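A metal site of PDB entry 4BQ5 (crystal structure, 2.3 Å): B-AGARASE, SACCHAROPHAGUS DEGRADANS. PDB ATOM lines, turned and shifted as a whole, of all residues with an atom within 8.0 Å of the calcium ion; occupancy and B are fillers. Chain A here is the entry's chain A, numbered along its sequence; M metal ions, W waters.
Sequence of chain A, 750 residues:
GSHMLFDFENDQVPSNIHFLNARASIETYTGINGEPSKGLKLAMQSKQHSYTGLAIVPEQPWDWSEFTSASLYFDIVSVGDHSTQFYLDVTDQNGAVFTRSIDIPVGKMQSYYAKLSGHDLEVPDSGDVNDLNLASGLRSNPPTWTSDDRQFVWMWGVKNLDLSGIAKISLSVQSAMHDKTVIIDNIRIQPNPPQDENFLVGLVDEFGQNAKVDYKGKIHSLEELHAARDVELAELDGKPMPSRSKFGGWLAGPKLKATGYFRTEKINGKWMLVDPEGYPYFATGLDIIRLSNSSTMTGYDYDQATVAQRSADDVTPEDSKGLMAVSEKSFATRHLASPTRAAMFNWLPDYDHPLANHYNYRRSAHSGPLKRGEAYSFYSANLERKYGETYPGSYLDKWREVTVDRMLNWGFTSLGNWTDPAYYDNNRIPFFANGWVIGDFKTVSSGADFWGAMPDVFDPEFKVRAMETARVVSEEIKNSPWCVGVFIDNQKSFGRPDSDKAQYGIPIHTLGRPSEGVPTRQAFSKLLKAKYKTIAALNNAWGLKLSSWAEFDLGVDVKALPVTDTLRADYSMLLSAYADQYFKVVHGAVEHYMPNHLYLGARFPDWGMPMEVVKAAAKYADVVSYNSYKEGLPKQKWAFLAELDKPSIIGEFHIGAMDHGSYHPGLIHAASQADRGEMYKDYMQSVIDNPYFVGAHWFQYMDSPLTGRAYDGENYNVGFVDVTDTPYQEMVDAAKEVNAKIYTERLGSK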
ATOM      1  N   HIS A 353     -10.948 -29.795  -6.671  1.00  0.00           N
ATOM      2  CA  HIS A 353      -9.568 -29.739  -6.164  1.00  0.00           C
ATOM      3  C   HIS A 353      -9.522 -29.007  -4.807  1.00  0.00           C
ATOM      4  O   HIS A 353     -10.207 -27.997  -4.655  1.00  0.00           O
ATOM      5  CB  HIS A 353      -8.669 -29.048  -7.190  1.00  0.00           C
ATOM      6  CG  HIS A 353      -7.200 -29.107  -6.869  1.00  0.00           C
ATOM      7  ND1 HIS A 353      -6.618 -28.315  -5.910  1.00  0.00           N
ATOM      8  CD2 HIS A 353      -6.215 -29.862  -7.388  1.00  0.00           C
ATOM      9  CE1 HIS A 353      -5.322 -28.582  -5.858  1.00  0.00           C
ATOM     10  NE2 HIS A 353      -5.055 -29.525  -6.739  1.00  0.00           N
ATOM     11  N   PRO A 354      -8.716 -29.504  -3.832  1.00  0.00           N
ATOM     12  CA  PRO A 354      -8.672 -28.881  -2.483  1.00  0.00           C
ATOM     13  C   PRO A 354      -8.552 -27.362  -2.488  1.00  0.00           C
ATOM     14  O   PRO A 354      -9.094 -26.705  -1.604  1.00  0.00           O
ATOM     15  CB  PRO A 354      -7.429 -29.503  -1.816  1.00  0.00           C
ATOM     16  CG  PRO A 354      -6.739 -30.299  -2.890  1.00  0.00           C
ATOM     17  CD  PRO A 354      -7.780 -30.633  -3.920  1.00  0.00           C
ATOM     18  N   LEU A 355      -7.848 -26.822  -3.490  1.00  0.00           N
ATOM     19  CA  LEU A 355      -7.532 -25.379  -3.565  1.00  0.00           C
ATOM     20  C   LEU A 355      -8.544 -24.538  -4.378  1.00  0.00           C
ATOM     21  O   LEU A 355      -8.393 -23.328  -4.513  1.00  0.00           O
ATOM     22  CB  LEU A 355      -6.063 -25.154  -4.023  1.00  0.00           C
ATOM     23  CG  LEU A 355      -4.930 -25.752  -3.151  1.00  0.00           C
ATOM     24  CD1 LEU A 355      -3.535 -25.385  -3.611  1.00  0.00           C
ATOM     25  CD2 LEU A 355      -5.064 -25.421  -1.668  1.00  0.00           C
ATOM     26  N   ALA A 356      -9.604 -25.205  -4.853  1.00  0.00           N
ATOM     27  CA  ALA A 356     -10.737 -24.542  -5.531  1.00  0.00           C
ATOM     28  C   ALA A 356     -11.507 -23.497  -4.725  1.00  0.00           C
ATOM     29  O   ALA A 356     -12.198 -22.654  -5.329  1.00  0.00           O
ATOM     30  CB  ALA A 356     -11.715 -25.585  -6.048  1.00  0.00           C
ATOM     31  N   ASN A 357     -11.427 -23.515  -3.402  1.00  0.00           N
ATOM     32  CA  ASN A 357     -12.051 -22.415  -2.652  1.00  0.00           C
ATOM     33  C   ASN A 357     -11.368 -21.041  -2.795  1.00  0.00           C
ATOM     34  O   ASN A 357     -11.875 -20.058  -2.290  1.00  0.00           O
ATOM     35  CB  ASN A 357     -12.201 -22.749  -1.166  1.00  0.00           C
ATOM     36  CG  ASN A 357     -10.885 -23.091  -0.524  1.00  0.00           C
ATOM     37  OD1 ASN A 357     -10.263 -24.092  -0.869  1.00  0.00           O
ATOM     38  ND2 ASN A 357     -10.434 -22.248   0.398  1.00  0.00           N
ATOM     39  N   HIS A 358     -10.234 -20.962  -3.470  1.00  0.00           N
ATOM     40  CA  HIS A 358      -9.556 -19.663  -3.571  1.00  0.00           C
ATOM     41  C   HIS A 358      -9.899 -18.897  -4.868  1.00  0.00           C
ATOM     42  O   HIS A 358      -9.207 -17.960  -5.297  1.00  0.00           O
ATOM     43  CB  HIS A 358      -8.064 -19.836  -3.350  1.00  0.00           C
ATOM     44  CG  HIS A 358      -7.743 -20.585  -2.105  1.00  0.00           C
ATOM     45  ND1 HIS A 358      -7.622 -19.979  -0.881  1.00  0.00           N
ATOM     46  CD2 HIS A 358      -7.588 -21.919  -1.886  1.00  0.00           C
ATOM     47  CE1 HIS A 358      -7.370 -20.890   0.035  1.00  0.00           C
ATOM     48  NE2 HIS A 358      -7.347 -22.073  -0.539  1.00  0.00           N
ATOM     49  N   ALA A 381      -4.495 -19.430  -1.720  1.00  0.00           N
ATOM     50  CA  ALA A 381      -4.136 -20.844  -1.982  1.00  0.00           C
ATOM     51  C   ALA A 381      -2.892 -21.289  -1.230  1.00  0.00           C
ATOM     52  O   ALA A 381      -2.896 -22.393  -0.651  1.00  0.00           O
ATOM     53  CB  ALA A 381      -3.970 -21.115  -3.467  1.00  0.00           C
ATOM     54  N   GLU A 384      -3.206 -22.001   2.469  1.00  0.00           N
ATOM     55  CA  GLU A 384      -3.722 -23.316   2.711  1.00  0.00           C
ATOM     56  C   GLU A 384      -2.649 -24.387   2.440  1.00  0.00           C
ATOM     57  O   GLU A 384      -2.452 -25.259   3.294  1.00  0.00           O
ATOM     58  CB  GLU A 384      -4.974 -23.546   1.909  1.00  0.00           C
ATOM     59  CG  GLU A 384      -5.363 -25.001   1.815  1.00  0.00           C
ATOM     60  CD  GLU A 384      -6.781 -25.157   1.356  1.00  0.00           C
ATOM     61  OE1 GLU A 384      -7.257 -24.248   0.624  1.00  0.00           O
ATOM     62  OE2 GLU A 384      -7.414 -26.165   1.715  1.00  0.00           O
ATOM     63  N   ARG A 385      -1.914 -24.291   1.313  1.00  0.00           N
ATOM     64  CA  ARG A 385      -0.746 -25.178   1.090  1.00  0.00           C
ATOM     65  C   ARG A 385       0.157 -25.216   2.306  1.00  0.00           C
ATOM     66  O   ARG A 385       0.574 -26.317   2.725  1.00  0.00           O
ATOM     67  CB  ARG A 385       0.139 -24.747  -0.100  1.00  0.00           C
ATOM     68  CG  ARG A 385      -0.470 -24.950  -1.475  1.00  0.00           C
ATOM     69  CD  ARG A 385       0.445 -24.459  -2.575  1.00  0.00           C
ATOM     70  NE  ARG A 385      -0.062 -24.988  -3.815  1.00  0.00           N
ATOM     71  CZ  ARG A 385      -0.429 -24.257  -4.872  1.00  0.00           C
ATOM     72  NH1 ARG A 385      -0.309 -22.926  -4.865  1.00  0.00           N
ATOM     73  NH2 ARG A 385      -0.922 -24.874  -5.949  1.00  0.00           N
ATOM     74  N   GLY A 388      -2.502 -26.012   5.863  1.00  0.00           N
ATOM     75  CA  GLY A 388      -3.541 -27.035   5.802  1.00  0.00           C
ATOM     76  C   GLY A 388      -4.901 -26.514   6.235  1.00  0.00           C
ATOM     77  O   GLY A 388      -5.070 -25.362   6.670  1.00  0.00           O
ATOM     78  N   GLU A 389      -5.900 -27.378   6.127  1.00  0.00           N
ATOM     79  CA  GLU A 389      -7.227 -26.963   6.490  1.00  0.00           C
ATOM     80  C   GLU A 389      -7.820 -28.049   7.325  1.00  0.00           C
ATOM     81  O   GLU A 389      -8.510 -28.914   6.796  1.00  0.00           O
ATOM     82  CB  GLU A 389      -8.068 -26.754   5.231  1.00  0.00           C
ATOM     83  CG  GLU A 389      -9.320 -25.917   5.444  1.00  0.00           C
ATOM     84  CD  GLU A 389     -10.422 -26.272   4.478  1.00  0.00           C
ATOM     85  OE1 GLU A 389     -10.454 -27.426   3.985  1.00  0.00           O
ATOM     86  OE2 GLU A 389     -11.272 -25.387   4.199  1.00  0.00           O
ATOM     87  N   TYR A 391     -10.153 -27.584   9.840  1.00  0.00           N
ATOM     88  CA  TYR A 391     -11.590 -27.308   9.809  1.00  0.00           C
ATOM     89  C   TYR A 391     -11.655 -26.216   8.762  1.00  0.00           C
ATOM     90  O   TYR A 391     -10.663 -25.577   8.514  1.00  0.00           O
ATOM     91  CB  TYR A 391     -12.133 -26.826  11.193  1.00  0.00           C
ATOM     92  CG  TYR A 391     -11.382 -25.646  11.782  1.00  0.00           C
ATOM     93  CD1 TYR A 391     -11.649 -24.322  11.362  1.00  0.00           C
ATOM     94  CD2 TYR A 391     -10.362 -25.845  12.731  1.00  0.00           C
ATOM     95  CE1 TYR A 391     -10.928 -23.241  11.894  1.00  0.00           C
ATOM     96  CE2 TYR A 391      -9.637 -24.762  13.251  1.00  0.00           C
ATOM     97  CZ  TYR A 391      -9.923 -23.468  12.826  1.00  0.00           C
ATOM     98  OH  TYR A 391      -9.188 -22.425  13.344  1.00  0.00           O
ATOM     99  N   PRO A 392     -12.839 -25.998   8.141  1.00  0.00           N
ATOM    100  CA  PRO A 392     -12.860 -25.021   7.050  1.00  0.00           C
ATOM    101  C   PRO A 392     -12.273 -23.652   7.414  1.00  0.00           C
ATOM    102  O   PRO A 392     -12.692 -22.987   8.373  1.00  0.00           O
ATOM    103  CB  PRO A 392     -14.345 -24.912   6.692  1.00  0.00           C
ATOM    104  CG  PRO A 392     -14.928 -26.241   7.121  1.00  0.00           C
ATOM    105  CD  PRO A 392     -14.144 -26.668   8.335  1.00  0.00           C
ATOM    106  N   GLY A 393     -11.297 -23.247   6.619  1.00  0.00           N
ATOM    107  CA  GLY A 393     -10.703 -21.931   6.748  1.00  0.00           C
ATOM    108  C   GLY A 393      -9.742 -21.779   7.898  1.00  0.00           C
ATOM    109  O   GLY A 393      -9.453 -20.657   8.268  1.00  0.00           O
ATOM    110  N   TYR A 395      -6.607 -22.274   8.074  1.00  0.00           N
ATOM    111  CA  TYR A 395      -5.375 -21.654   7.628  1.00  0.00           C
ATOM    112  C   TYR A 395      -5.529 -20.135   7.765  1.00  0.00           C
ATOM    113  O   TYR A 395      -4.528 -19.444   7.866  1.00  0.00           O
ATOM    114  CB  TYR A 395      -5.035 -22.025   6.169  1.00  0.00           C
ATOM    115  CG  TYR A 395      -6.196 -21.839   5.231  1.00  0.00           C
ATOM    116  CD1 TYR A 395      -7.082 -22.890   5.019  1.00  0.00           C
ATOM    117  CD2 TYR A 395      -6.430 -20.621   4.578  1.00  0.00           C
ATOM    118  CE1 TYR A 395      -8.167 -22.744   4.198  1.00  0.00           C
ATOM    119  CE2 TYR A 395      -7.539 -20.462   3.741  1.00  0.00           C
ATOM    120  CZ  TYR A 395      -8.403 -21.552   3.572  1.00  0.00           C
ATOM    121  OH  TYR A 395      -9.504 -21.494   2.756  1.00  0.00           O
HETATM  122 CA    CA M   1      -9.662 -25.915   0.851  1.00  0.00          CA
HETATM  123  O   HOH W   1     -11.603 -26.742  -0.136  1.00  0.00           O
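Merely in contact with the calcium ion: Glu 389 (3.6 Å).
Four residues have an atom within 4 Å of the calcium ion: Pro 354, Asn 357, Glu 384 and Glu 389.
The nearest printed residue that does not touch the calcium ion is His 358 (4.7 Å).
OE1 of Glu 384 is in hydrogen-bond range of NE2 of His 358, at 2.5 Å.
The side-chain amide nitrogen (ND2) of Asn 357 lies within hydrogen-bond range of a ring nitrogen (NE2) of His 358, 3.2 Å away.
ND2 of Asn 357 lies within hydrogen-bond range of OH of Tyr 395.
N of Gly 393 lies within hydrogen-bond range of OE2 of Glu 389 (3.2 Å).
The calcium ion is bound by water W1 (2.3 Å), the side-chain carboxylate of Glu 384 (2.4 Å), the side-chain amide oxygen of Asn 357 (2.6 Å) and the backbone carbonyl oxygen of Pro 354 (2.6 Å).
The calcium ion has four donor atoms within binding distance.
Slightly farther from the calcium ion lies OE1 of Glu 384 (2.9 Å).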
